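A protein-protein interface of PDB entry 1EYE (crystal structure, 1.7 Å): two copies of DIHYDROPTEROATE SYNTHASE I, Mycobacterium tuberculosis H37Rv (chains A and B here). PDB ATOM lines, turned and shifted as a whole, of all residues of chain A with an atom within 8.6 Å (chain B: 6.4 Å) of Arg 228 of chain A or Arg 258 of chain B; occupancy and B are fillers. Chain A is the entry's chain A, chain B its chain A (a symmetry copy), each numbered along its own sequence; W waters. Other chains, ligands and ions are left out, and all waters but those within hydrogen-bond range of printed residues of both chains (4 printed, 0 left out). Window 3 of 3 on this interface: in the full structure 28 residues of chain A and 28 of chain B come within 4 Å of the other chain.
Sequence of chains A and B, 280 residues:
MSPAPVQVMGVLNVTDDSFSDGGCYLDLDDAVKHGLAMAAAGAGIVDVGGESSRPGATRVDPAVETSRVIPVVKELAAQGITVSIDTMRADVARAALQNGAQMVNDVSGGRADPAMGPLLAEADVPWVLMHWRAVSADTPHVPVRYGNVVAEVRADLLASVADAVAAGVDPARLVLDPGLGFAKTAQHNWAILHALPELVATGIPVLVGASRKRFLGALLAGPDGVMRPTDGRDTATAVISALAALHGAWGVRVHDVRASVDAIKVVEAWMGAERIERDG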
ATOM      1  N   ARG A 212      10.897   7.743  25.477  1.00  0.00           N
ATOM      2  CA  ARG A 212       9.817   8.116  24.585  1.00  0.00           C
ATOM      3  C   ARG A 212       9.811   7.488  23.211  1.00  0.00           C
ATOM      4  O   ARG A 212       9.073   7.954  22.353  1.00  0.00           O
ATOM      5  CB  ARG A 212       9.695   9.617  24.466  1.00  0.00           C
ATOM      6  CG  ARG A 212       9.629  10.306  25.833  1.00  0.00           C
ATOM      7  CD  ARG A 212       9.484  11.817  25.672  1.00  0.00           C
ATOM      8  NE  ARG A 212       9.181  12.498  26.916  1.00  0.00           N
ATOM      9  CZ  ARG A 212       8.886  13.781  26.897  1.00  0.00           C
ATOM     10  NH1 ARG A 212       8.878  14.433  25.735  1.00  0.00           N
ATOM     11  NH2 ARG A 212       8.588  14.420  28.034  1.00  0.00           N
ATOM     12  N   LYS A 213      10.620   6.463  23.009  1.00  0.00           N
ATOM     13  CA  LYS A 213      10.682   5.870  21.687  1.00  0.00           C
ATOM     14  C   LYS A 213       9.392   5.180  21.281  1.00  0.00           C
ATOM     15  O   LYS A 213       8.537   4.873  22.112  1.00  0.00           O
ATOM     16  CB  LYS A 213      11.927   5.010  21.511  1.00  0.00           C
ATOM     17  CG  LYS A 213      13.226   5.802  21.329  1.00  0.00           C
ATOM     18  CD  LYS A 213      14.442   4.903  21.008  1.00  0.00           C
ATOM     19  CE  LYS A 213      15.721   5.638  20.567  1.00  0.00           C
ATOM     20  NZ  LYS A 213      16.395   6.353  21.678  1.00  0.00           N
ATOM     21  N   ARG A 214       9.256   4.946  19.977  1.00  0.00           N
ATOM     22  CA  ARG A 214       8.082   4.323  19.380  1.00  0.00           C
ATOM     23  C   ARG A 214       7.621   3.078  20.113  1.00  0.00           C
ATOM     24  O   ARG A 214       6.423   2.882  20.334  1.00  0.00           O
ATOM     25  CB  ARG A 214       8.309   3.983  17.892  1.00  0.00           C
ATOM     26  CG  ARG A 214       7.045   3.980  17.048  1.00  0.00           C
ATOM     27  CD  ARG A 214       6.765   2.663  16.324  1.00  0.00           C
ATOM     28  NE  ARG A 214       6.045   2.801  15.042  1.00  0.00           N
ATOM     29  CZ  ARG A 214       5.311   3.832  14.571  1.00  0.00           C
ATOM     30  NH1 ARG A 214       5.114   4.983  15.212  1.00  0.00           N
ATOM     31  NH2 ARG A 214       4.750   3.699  13.368  1.00  0.00           N
ATOM     32  N   PHE A 215       8.570   2.201  20.439  1.00  0.00           N
ATOM     33  CA  PHE A 215       8.208   0.964  21.109  1.00  0.00           C
ATOM     34  C   PHE A 215       7.344   1.194  22.349  1.00  0.00           C
ATOM     35  O   PHE A 215       6.509   0.360  22.712  1.00  0.00           O
ATOM     36  CB  PHE A 215       9.388  -0.041  21.302  1.00  0.00           C
ATOM     37  CG  PHE A 215      10.326   0.177  22.489  1.00  0.00           C
ATOM     38  CD1 PHE A 215      10.545  -0.833  23.431  1.00  0.00           C
ATOM     39  CD2 PHE A 215      11.009   1.378  22.685  1.00  0.00           C
ATOM     40  CE1 PHE A 215      11.400  -0.669  24.521  1.00  0.00           C
ATOM     41  CE2 PHE A 215      11.881   1.561  23.759  1.00  0.00           C
ATOM     42  CZ  PHE A 215      12.078   0.537  24.688  1.00  0.00           C
ATOM     43  N   LEU A 216       7.572   2.317  23.023  1.00  0.00           N
ATOM     44  CA  LEU A 216       6.825   2.620  24.220  1.00  0.00           C
ATOM     45  C   LEU A 216       5.445   3.127  23.844  1.00  0.00           C
ATOM     46  O   LEU A 216       4.440   2.890  24.542  1.00  0.00           O
ATOM     47  CB  LEU A 216       7.580   3.598  25.141  1.00  0.00           C
ATOM     48  CG  LEU A 216       8.928   3.066  25.662  1.00  0.00           C
ATOM     49  CD1 LEU A 216       9.643   4.174  26.454  1.00  0.00           C
ATOM     50  CD2 LEU A 216       8.704   1.858  26.583  1.00  0.00           C
ATOM     51  N   GLY A 217       5.381   3.842  22.718  1.00  0.00           N
ATOM     52  CA  GLY A 217       4.087   4.340  22.254  1.00  0.00           C
ATOM     53  C   GLY A 217       3.152   3.168  21.970  1.00  0.00           C
ATOM     54  O   GLY A 217       1.942   3.209  22.236  1.00  0.00           O
ATOM     55  N   ALA A 218       3.759   2.110  21.428  1.00  0.00           N
ATOM     56  CA  ALA A 218       3.095   0.862  21.052  1.00  0.00           C
ATOM     57  C   ALA A 218       2.724   0.014  22.283  1.00  0.00           C
ATOM     58  O   ALA A 218       1.609  -0.508  22.436  1.00  0.00           O
ATOM     59  CB  ALA A 218       4.030   0.118  20.105  1.00  0.00           C
ATOM     60  N   LEU A 219       3.679  -0.114  23.182  1.00  0.00           N
ATOM     61  CA  LEU A 219       3.452  -0.847  24.399  1.00  0.00           C
ATOM     62  C   LEU A 219       2.232  -0.283  25.111  1.00  0.00           C
ATOM     63  O   LEU A 219       1.391  -1.009  25.636  1.00  0.00           O
ATOM     64  CB  LEU A 219       4.674  -0.711  25.353  1.00  0.00           C
ATOM     65  CG  LEU A 219       4.451  -1.395  26.711  1.00  0.00           C
ATOM     66  CD1 LEU A 219       4.501  -2.913  26.560  1.00  0.00           C
ATOM     67  CD2 LEU A 219       5.511  -0.984  27.713  1.00  0.00           C
ATOM     68  N   LEU A 220       2.168   1.042  25.158  1.00  0.00           N
ATOM     69  CA  LEU A 220       1.100   1.739  25.870  1.00  0.00           C
ATOM     70  C   LEU A 220      -0.068   2.222  25.025  1.00  0.00           C
ATOM     71  O   LEU A 220      -0.789   3.169  25.398  1.00  0.00           O
ATOM     72  CB  LEU A 220       1.713   2.919  26.667  1.00  0.00           C
ATOM     73  CG  LEU A 220       2.895   2.517  27.568  1.00  0.00           C
ATOM     74  CD1 LEU A 220       3.511   3.770  28.203  1.00  0.00           C
ATOM     75  CD2 LEU A 220       2.466   1.519  28.639  1.00  0.00           C
ATOM     76  N   ALA A 221      -0.258   1.605  23.872  1.00  0.00           N
ATOM     77  CA  ALA A 221      -1.334   2.058  23.015  1.00  0.00           C
ATOM     78  C   ALA A 221      -2.668   2.007  23.736  1.00  0.00           C
ATOM     79  O   ALA A 221      -2.855   1.134  24.588  1.00  0.00           O
ATOM     80  CB  ALA A 221      -1.402   1.247  21.748  1.00  0.00           C
ATOM     81  N   GLY A 222      -3.552   2.951  23.389  1.00  0.00           N
ATOM     82  CA  GLY A 222      -4.895   3.089  23.947  1.00  0.00           C
ATOM     83  C   GLY A 222      -5.814   1.923  23.584  1.00  0.00           C
ATOM     84  O   GLY A 222      -5.484   1.008  22.821  1.00  0.00           O
ATOM     85  N   PRO A 223      -6.996   1.917  24.178  1.00  0.00           N
ATOM     86  CA  PRO A 223      -7.937   0.841  23.916  1.00  0.00           C
ATOM     87  C   PRO A 223      -8.108   0.655  22.424  1.00  0.00           C
ATOM     88  O   PRO A 223      -8.062  -0.478  21.939  1.00  0.00           O
ATOM     89  CB  PRO A 223      -9.263   1.259  24.538  1.00  0.00           C
ATOM     90  CG  PRO A 223      -9.072   2.671  25.074  1.00  0.00           C
ATOM     91  CD  PRO A 223      -7.611   3.049  24.896  1.00  0.00           C
ATOM     92  N   ASP A 224      -8.289   1.793  21.735  1.00  0.00           N
ATOM     93  CA  ASP A 224      -8.473   1.873  20.290  1.00  0.00           C
ATOM     94  C   ASP A 224      -7.348   1.183  19.543  1.00  0.00           C
ATOM     95  O   ASP A 224      -7.554   0.351  18.660  1.00  0.00           O
ATOM     96  CB  ASP A 224      -8.479   3.344  19.863  1.00  0.00           C
ATOM     97  CG  ASP A 224      -7.458   4.109  20.662  1.00  0.00           C
ATOM     98  OD1 ASP A 224      -6.611   3.592  21.388  1.00  0.00           O
ATOM     99  OD2 ASP A 224      -7.577   5.398  20.497  1.00  0.00           O
ATOM    100  N   GLY A 225      -6.137   1.550  19.915  1.00  0.00           N
ATOM    101  CA  GLY A 225      -4.965   0.992  19.277  1.00  0.00           C
ATOM    102  C   GLY A 225      -4.060   2.150  18.896  1.00  0.00           C
ATOM    103  O   GLY A 225      -3.050   1.973  18.214  1.00  0.00           O
ATOM    104  N   VAL A 226      -4.473   3.335  19.349  1.00  0.00           N
ATOM    105  CA  VAL A 226      -3.731   4.555  19.115  1.00  0.00           C
ATOM    106  C   VAL A 226      -2.602   4.655  20.133  1.00  0.00           C
ATOM    107  O   VAL A 226      -2.792   4.515  21.341  1.00  0.00           O
ATOM    108  CB  VAL A 226      -4.622   5.783  19.116  1.00  0.00           C
ATOM    109  CG1 VAL A 226      -3.807   7.065  19.080  1.00  0.00           C
ATOM    110  CG2 VAL A 226      -5.562   5.729  17.921  1.00  0.00           C
ATOM    111  N   MET A 227      -1.407   4.884  19.607  1.00  0.00           N
ATOM    112  CA  MET A 227      -0.203   4.960  20.413  1.00  0.00           C
ATOM    113  C   MET A 227      -0.290   6.011  21.492  1.00  0.00           C
ATOM    114  O   MET A 227      -0.905   7.068  21.333  1.00  0.00           O
ATOM    115  CB  MET A 227       1.072   5.211  19.558  1.00  0.00           C
ATOM    116  CG  MET A 227       1.543   4.035  18.688  1.00  0.00           C
ATOM    117  SD  MET A 227       3.350   4.027  18.308  1.00  0.00           S
ATOM    118  CE  MET A 227       3.569   5.608  17.465  1.00  0.00           C
ATOM    119  N   ARG A 228       0.371   5.712  22.601  1.00  0.00           N
ATOM    120  CA  ARG A 228       0.440   6.679  23.674  1.00  0.00           C
ATOM    121  C   ARG A 228       1.239   7.863  23.134  1.00  0.00           C
ATOM    122  O   ARG A 228       2.260   7.645  22.511  1.00  0.00           O
ATOM    123  CB  ARG A 228       1.222   6.051  24.852  1.00  0.00           C
ATOM    124  CG  ARG A 228       1.336   6.977  26.057  1.00  0.00           C
ATOM    125  CD  ARG A 228      -0.034   7.259  26.714  1.00  0.00           C
ATOM    126  NE  ARG A 228      -0.612   6.054  27.325  1.00  0.00           N
ATOM    127  CZ  ARG A 228      -0.215   5.587  28.508  1.00  0.00           C
ATOM    128  NH1 ARG A 228       0.719   6.207  29.240  1.00  0.00           N
ATOM    129  NH2 ARG A 228      -0.758   4.454  28.974  1.00  0.00           N
ATOM    130  N   PRO A 229       0.849   9.113  23.388  1.00  0.00           N
ATOM    131  CA  PRO A 229       1.612  10.257  22.920  1.00  0.00           C
ATOM    132  C   PRO A 229       2.956  10.297  23.561  1.00  0.00           C
ATOM    133  O   PRO A 229       3.124   9.727  24.633  1.00  0.00           O
ATOM    134  CB  PRO A 229       0.833  11.497  23.336  1.00  0.00           C
ATOM    135  CG  PRO A 229      -0.605  11.008  23.417  1.00  0.00           C
ATOM    136  CD  PRO A 229      -0.545   9.521  23.714  1.00  0.00           C
ATOM    137  N   THR A 230       3.894  10.975  22.892  1.00  0.00           N
ATOM    138  CA  THR A 230       5.253  11.055  23.380  1.00  0.00           C
ATOM    139  C   THR A 230       5.356  11.452  24.833  1.00  0.00           C
ATOM    140  O   THR A 230       6.059  10.832  25.628  1.00  0.00           O
ATOM    141  CB  THR A 230       6.128  11.985  22.498  1.00  0.00           C
ATOM    142  OG1 THR A 230       5.546  13.263  22.384  1.00  0.00           O
ATOM    143  CG2 THR A 230       6.272  11.389  21.104  1.00  0.00           C
ATOM    144  N   ASP A 231       4.656  12.512  25.160  1.00  0.00           N
ATOM    145  CA  ASP A 231       4.646  13.043  26.508  1.00  0.00           C
ATOM    146  C   ASP A 231       4.111  12.038  27.519  1.00  0.00           C
ATOM    147  O   ASP A 231       4.353  12.192  28.699  1.00  0.00           O
ATOM    148  CB  ASP A 231       3.750  14.294  26.531  1.00  0.00           C
ATOM    149  CG  ASP A 231       4.532  15.534  26.781  1.00  0.00           C
ATOM    150  OD1 ASP A 231       4.879  15.874  27.897  1.00  0.00           O
ATOM    151  OD2 ASP A 231       4.785  16.199  25.681  1.00  0.00           O
ATOM    152  N   GLY A 232       3.344  11.046  27.069  1.00  0.00           N
ATOM    153  CA  GLY A 232       2.780  10.058  27.957  1.00  0.00           C
ATOM    154  C   GLY A 232       3.663   8.842  28.119  1.00  0.00           C
ATOM    155  O   GLY A 232       3.261   7.874  28.745  1.00  0.00           O
ATOM    156  N   ARG A 233       4.880   8.889  27.562  1.00  0.00           N
ATOM    157  CA  ARG A 233       5.760   7.736  27.666  1.00  0.00           C
ATOM    158  C   ARG A 233       6.804   7.900  28.746  1.00  0.00           C
ATOM    159  O   ARG A 233       7.706   7.076  28.843  1.00  0.00           O
ATOM    160  CB  ARG A 233       6.477   7.452  26.332  1.00  0.00           C
ATOM    161  CG  ARG A 233       5.492   7.304  25.190  1.00  0.00           C
ATOM    162  CD  ARG A 233       6.115   7.312  23.794  1.00  0.00           C
ATOM    163  NE  ARG A 233       5.100   7.468  22.726  1.00  0.00           N
ATOM    164  CZ  ARG A 233       5.402   7.507  21.421  1.00  0.00           C
ATOM    165  NH1 ARG A 233       6.656   7.379  20.989  1.00  0.00           N
ATOM    166  NH2 ARG A 233       4.436   7.646  20.525  1.00  0.00           N
ATOM    167  N   ASP A 234       6.711   8.946  29.554  1.00  0.00           N
ATOM    168  CA  ASP A 234       7.729   9.126  30.580  1.00  0.00           C
ATOM    169  C   ASP A 234       7.707   8.142  31.730  1.00  0.00           C
ATOM    170  O   ASP A 234       8.760   7.755  32.207  1.00  0.00           O
ATOM    171  CB  ASP A 234       7.824  10.565  31.087  1.00  0.00           C
ATOM    172  CG  ASP A 234       8.273  11.483  29.977  1.00  0.00           C
ATOM    173  OD1 ASP A 234       9.107  11.175  29.140  1.00  0.00           O
ATOM    174  OD2 ASP A 234       7.646  12.628  30.007  1.00  0.00           O
ATOM    175  N   THR A 235       6.528   7.739  32.192  1.00  0.00           N
ATOM    176  CA  THR A 235       6.521   6.780  33.291  1.00  0.00           C
ATOM    177  C   THR A 235       7.235   5.508  32.848  1.00  0.00           C
ATOM    178  O   THR A 235       8.106   4.986  33.557  1.00  0.00           O
ATOM    179  CB  THR A 235       5.097   6.471  33.841  1.00  0.00           C
ATOM    180  OG1 THR A 235       4.467   7.689  34.129  1.00  0.00           O
ATOM    181  CG2 THR A 235       5.222   5.675  35.128  1.00  0.00           C
ATOM    182  N   ALA A 236       6.858   5.012  31.674  1.00  0.00           N
ATOM    183  CA  ALA A 236       7.497   3.810  31.127  1.00  0.00           C
ATOM    184  C   ALA A 236       9.006   3.999  31.009  1.00  0.00           C
ATOM    185  O   ALA A 236       9.815   3.114  31.355  1.00  0.00           O
ATOM    186  CB  ALA A 236       6.878   3.423  29.788  1.00  0.00           C
ATOM    187  N   ALA B  41      -8.609   2.475  32.880  1.00  0.00           N
ATOM    188  CA  ALA B  41      -7.162   2.534  32.827  1.00  0.00           C
ATOM    189  C   ALA B  41      -6.503   1.217  33.205  1.00  0.00           C
ATOM    190  O   ALA B  41      -5.291   1.111  33.128  1.00  0.00           O
ATOM    191  CB  ALA B  41      -6.619   3.650  33.685  1.00  0.00           C
ATOM    192  N   VAL B 254      -3.100   2.300  44.332  1.00  0.00           N
ATOM    193  CA  VAL B 254      -2.583   3.571  43.840  1.00  0.00           C
ATOM    194  C   VAL B 254      -3.620   4.605  43.437  1.00  0.00           C
ATOM    195  O   VAL B 254      -4.766   4.266  43.102  1.00  0.00           O
ATOM    196  CB  VAL B 254      -1.752   3.251  42.584  1.00  0.00           C
ATOM    197  CG1 VAL B 254      -0.739   2.146  42.880  1.00  0.00           C
ATOM    198  CG2 VAL B 254      -2.628   2.810  41.408  1.00  0.00           C
ATOM    199  N   HIS B 255      -3.182   5.866  43.400  1.00  0.00           N
ATOM    200  CA  HIS B 255      -4.062   6.957  42.948  1.00  0.00           C
ATOM    201  C   HIS B 255      -4.044   7.098  41.423  1.00  0.00           C
ATOM    202  O   HIS B 255      -5.080   7.256  40.793  1.00  0.00           O
ATOM    203  CB  HIS B 255      -3.684   8.310  43.539  1.00  0.00           C
ATOM    204  CG  HIS B 255      -3.703   8.248  45.029  1.00  0.00           C
ATOM    205  ND1 HIS B 255      -2.622   7.736  45.740  1.00  0.00           N
ATOM    206  CD2 HIS B 255      -4.680   8.611  45.905  1.00  0.00           C
ATOM    207  CE1 HIS B 255      -2.943   7.820  47.036  1.00  0.00           C
ATOM    208  NE2 HIS B 255      -4.184   8.321  47.156  1.00  0.00           N
ATOM    209  N   ASP B 256      -2.856   7.063  40.833  1.00  0.00           N
ATOM    210  CA  ASP B 256      -2.676   7.194  39.379  1.00  0.00           C
ATOM    211  C   ASP B 256      -2.528   5.818  38.786  1.00  0.00           C
ATOM    212  O   ASP B 256      -1.452   5.220  38.797  1.00  0.00           O
ATOM    213  CB  ASP B 256      -1.376   7.975  39.097  1.00  0.00           C
ATOM    214  CG  ASP B 256      -1.070   8.188  37.621  1.00  0.00           C
ATOM    215  OD1 ASP B 256      -1.627   7.617  36.703  1.00  0.00           O
ATOM    216  OD2 ASP B 256      -0.099   9.044  37.425  1.00  0.00           O
ATOM    217  N   VAL B 257      -3.651   5.305  38.322  1.00  0.00           N
ATOM    218  CA  VAL B 257      -3.714   3.991  37.766  1.00  0.00           C
ATOM    219  C   VAL B 257      -2.825   3.805  36.528  1.00  0.00           C
ATOM    220  O   VAL B 257      -2.058   2.845  36.406  1.00  0.00           O
ATOM    221  CB  VAL B 257      -5.178   3.654  37.486  1.00  0.00           C
ATOM    222  CG1 VAL B 257      -5.331   2.334  36.743  1.00  0.00           C
ATOM    223  CG2 VAL B 257      -5.911   3.538  38.827  1.00  0.00           C
ATOM    224  N   ARG B 258      -2.984   4.722  35.584  1.00  0.00           N
ATOM    225  CA  ARG B 258      -2.221   4.658  34.333  1.00  0.00           C
ATOM    226  C   ARG B 258      -0.755   4.494  34.588  1.00  0.00           C
ATOM    227  O   ARG B 258      -0.105   3.614  34.009  1.00  0.00           O
ATOM    228  CB  ARG B 258      -2.403   5.928  33.537  1.00  0.00           C
ATOM    229  CG  ARG B 258      -1.898   5.766  32.109  1.00  0.00           C
ATOM    230  CD  ARG B 258      -2.365   6.943  31.261  1.00  0.00           C
ATOM    231  NE  ARG B 258      -1.488   8.054  31.579  1.00  0.00           N
ATOM    232  CZ  ARG B 258      -1.027   8.899  30.659  1.00  0.00           C
ATOM    233  NH1 ARG B 258      -1.378   8.777  29.376  1.00  0.00           N
ATOM    234  NH2 ARG B 258      -0.202   9.883  31.031  1.00  0.00           N
ATOM    235  N   ALA B 259      -0.245   5.332  35.482  1.00  0.00           N
ATOM    236  CA  ALA B 259       1.166   5.276  35.809  1.00  0.00           C
ATOM    237  C   ALA B 259       1.613   3.891  36.291  1.00  0.00           C
ATOM    238  O   ALA B 259       2.608   3.339  35.796  1.00  0.00           O
ATOM    239  CB  ALA B 259       1.556   6.441  36.708  1.00  0.00           C
ATOM    240  N   SER B 260       0.880   3.307  37.252  1.00  0.00           N
ATOM    241  CA  SER B 260       1.261   1.992  37.737  1.00  0.00           C
ATOM    242  C   SER B 260       1.023   0.899  36.706  1.00  0.00           C
ATOM    243  O   SER B 260       1.766  -0.069  36.632  1.00  0.00           O
ATOM    244  CB  SER B 260       0.709   1.658  39.129  1.00  0.00           C
ATOM    245  OG  SER B 260       1.423   2.396  40.121  1.00  0.00           O
ATOM    246  N   VAL B 261      -0.029   1.028  35.894  1.00  0.00           N
ATOM    247  CA  VAL B 261      -0.274   0.027  34.869  1.00  0.00           C
ATOM    248  C   VAL B 261       0.858   0.086  33.825  1.00  0.00           C
ATOM    249  O   VAL B 261       1.346  -0.940  33.347  1.00  0.00           O
ATOM    250  CB  VAL B 261      -1.663   0.214  34.232  1.00  0.00           C
ATOM    251  CG1 VAL B 261      -1.846  -0.659  32.987  1.00  0.00           C
ATOM    252  CG2 VAL B 261      -2.760  -0.139  35.264  1.00  0.00           C
ATOM    253  N   ASP B 262       1.274   1.309  33.488  1.00  0.00           N
ATOM    254  CA  ASP B 262       2.369   1.509  32.541  1.00  0.00           C
ATOM    255  C   ASP B 262       3.615   0.767  33.034  1.00  0.00           C
ATOM    256  O   ASP B 262       4.264  -0.010  32.288  1.00  0.00           O
ATOM    257  CB  ASP B 262       2.685   3.021  32.423  1.00  0.00           C
ATOM    258  CG  ASP B 262       1.713   3.788  31.569  1.00  0.00           C
ATOM    259  OD1 ASP B 262       0.719   3.285  31.069  1.00  0.00           O
ATOM    260  OD2 ASP B 262       1.981   5.080  31.522  1.00  0.00           O
ATOM    261  N   ALA B 263       3.918   0.980  34.341  1.00  0.00           N
ATOM    262  CA  ALA B 263       5.075   0.361  34.977  1.00  0.00           C
ATOM    263  C   ALA B 263       5.044  -1.147  34.890  1.00  0.00           C
ATOM    264  O   ALA B 263       6.055  -1.791  34.625  1.00  0.00           O
ATOM    265  CB  ALA B 263       5.243   0.800  36.432  1.00  0.00           C
ATOM    266  N   LYS B 265       3.288  -2.958  32.722  1.00  0.00           N
ATOM    267  CA  LYS B 265       3.469  -3.385  31.335  1.00  0.00           C
ATOM    268  C   LYS B 265       4.970  -3.446  30.986  1.00  0.00           C
ATOM    269  O   LYS B 265       5.454  -4.385  30.329  1.00  0.00           O
ATOM    270  CB  LYS B 265       2.748  -2.432  30.384  1.00  0.00           C
ATOM    271  CG  LYS B 265       1.236  -2.459  30.544  1.00  0.00           C
ATOM    272  CD  LYS B 265       0.488  -1.555  29.580  1.00  0.00           C
ATOM    273  CE  LYS B 265      -1.024  -1.790  29.624  1.00  0.00           C
ATOM    274  NZ  LYS B 265      -1.795  -0.665  29.065  1.00  0.00           N
HETATM  275  O   HOH W   1       2.020   7.331  33.069  1.00  0.00           O
HETATM  276  O   HOH W   2       4.388   6.111  30.387  1.00  0.00           O
HETATM  277  O   HOH W   3      -1.222   1.643  30.662  1.00  0.00           O
HETATM  278  O   HOH W   4      -1.325  -0.402  26.305  1.00  0.00           O
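Water W3 lies within hydrogen-bond range of OD1 of Asp 262 of chain B, NZ of Lys 265 of chain B and NH2 of Arg 228 of chain A. Water W2 lies within hydrogen-bond range of the backbone carbonyl oxygen of Gly 232 of chain A (2.7 Å), the side-chain carboxylate of Asp 262 of chain B (2.9 Å), the backbone NH of Ala 236 of chain A (3.0 Å) and the backbone NH of Thr 235 of chain A (3.2 Å). Water W1 bridges OG1 of Thr 235 of chain A (2.7 Å) and OD2 of Asp 262 of chain B (2.7 Å). Water W4 lies within hydrogen-bond range of the backbone carbonyl oxygen of Ala 221 of chain A (2.8 Å), the side-chain amino group of Lys 265 of chain B (2.8 Å) and the backbone carbonyl oxygen of Leu 219 of chain A (2.9 Å).
Printed residues of chain B within 4 Å of Leu 220 of chain A: Asp 262 and Lys 265. Arg 228 of chain A touches just these residues of chain B: Arg 258 (3.3 Å) and Asp 262 (2.8 Å). Gly 232 of chain A touches none of the printed residues of chain B. Printed residues of chain B within 4 Å of Thr 235 of chain A: Ala 259 (3.6 Å). Ala 259 of chain B touches just one residue of chain A: Thr 235 (3.6 Å). Printed residues of chain A within 4 Å of Asp 262 of chain B: Leu 220 and Arg 228. The nearest residue of chain B that does not touch Arg 228 of chain A is Lys 265 of chain B (5.2 Å). The nearest residue of chain A that does not touch Arg 258 of chain B is Gly 232 of chain A (4.3 Å).
Of the 25 printed residues of chain A, 3 touch a printed residue of chain B. Hydrophobic or aromatic side chains of chain A within 4 Å of the printed part of chain B: Leu 220. Printed residues of chain B that touch a printed residue of chain A: Arg 258, Ala 259, Asp 262 and Lys 265. Among the printed residues, 5 pairs touch across the chains. Among the printed residues, Asp or Glu carboxylates within 4 Å of a Lys or Arg side-chain nitrogen of the other chain: Arg 228 of chain A with Asp 262 of chain B (2.8 Å).
No position is printed for both chains.
Leu 220 of chain A touches Asp 262 of chain B (CD2 to OD1, 3.5 Å). Lys 265 of chain B touches Leu 220 of chain A (CD to CD2, 3.8 Å). CG2 of Thr 235 of chain A touches O of Ala 259 of chain B (3.6 Å).
The guanidinium group of Arg 228 of chain A sits close to the guanidinium group of Arg 258 of chain B. OD1 of Asp 262 of chain B lies within salt-bridge range of NH2 of Arg 228 of chain A (2.8 Å).
The guanidinium group (NE) of Arg 233 of chain A sits at hydrogen-bond distance from the backbone carbonyl oxygen (O) of Arg 228 of chain A (2.9 Å). O of Gly 217 of chain A sits at hydrogen-bond distance from N of Arg 228 of chain A (3.0 Å). The backbone carbonyl oxygen (O) of Leu 220 of chain A lies within hydrogen-bond range of the guanidinium group (NE) of Arg 228 of chain A, at 3.5 Å. The side-chain carboxylate (OD1) of Asp 256 of chain B is in hydrogen-bond range of the backbone NH (N) of Arg 258 of chain B, 3.4 Å away. The side-chain carboxylate of Asp 256 of chain B is in hydrogen-bond range of the backbone NH of Ala 259 of chain B, at 2.9 Å. The backbone carbonyl oxygen (O) of Gly 232 of chain A is in hydrogen-bond range of the guanidinium group (NH1) of Arg 228 of chain A, 3.1 Å away.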
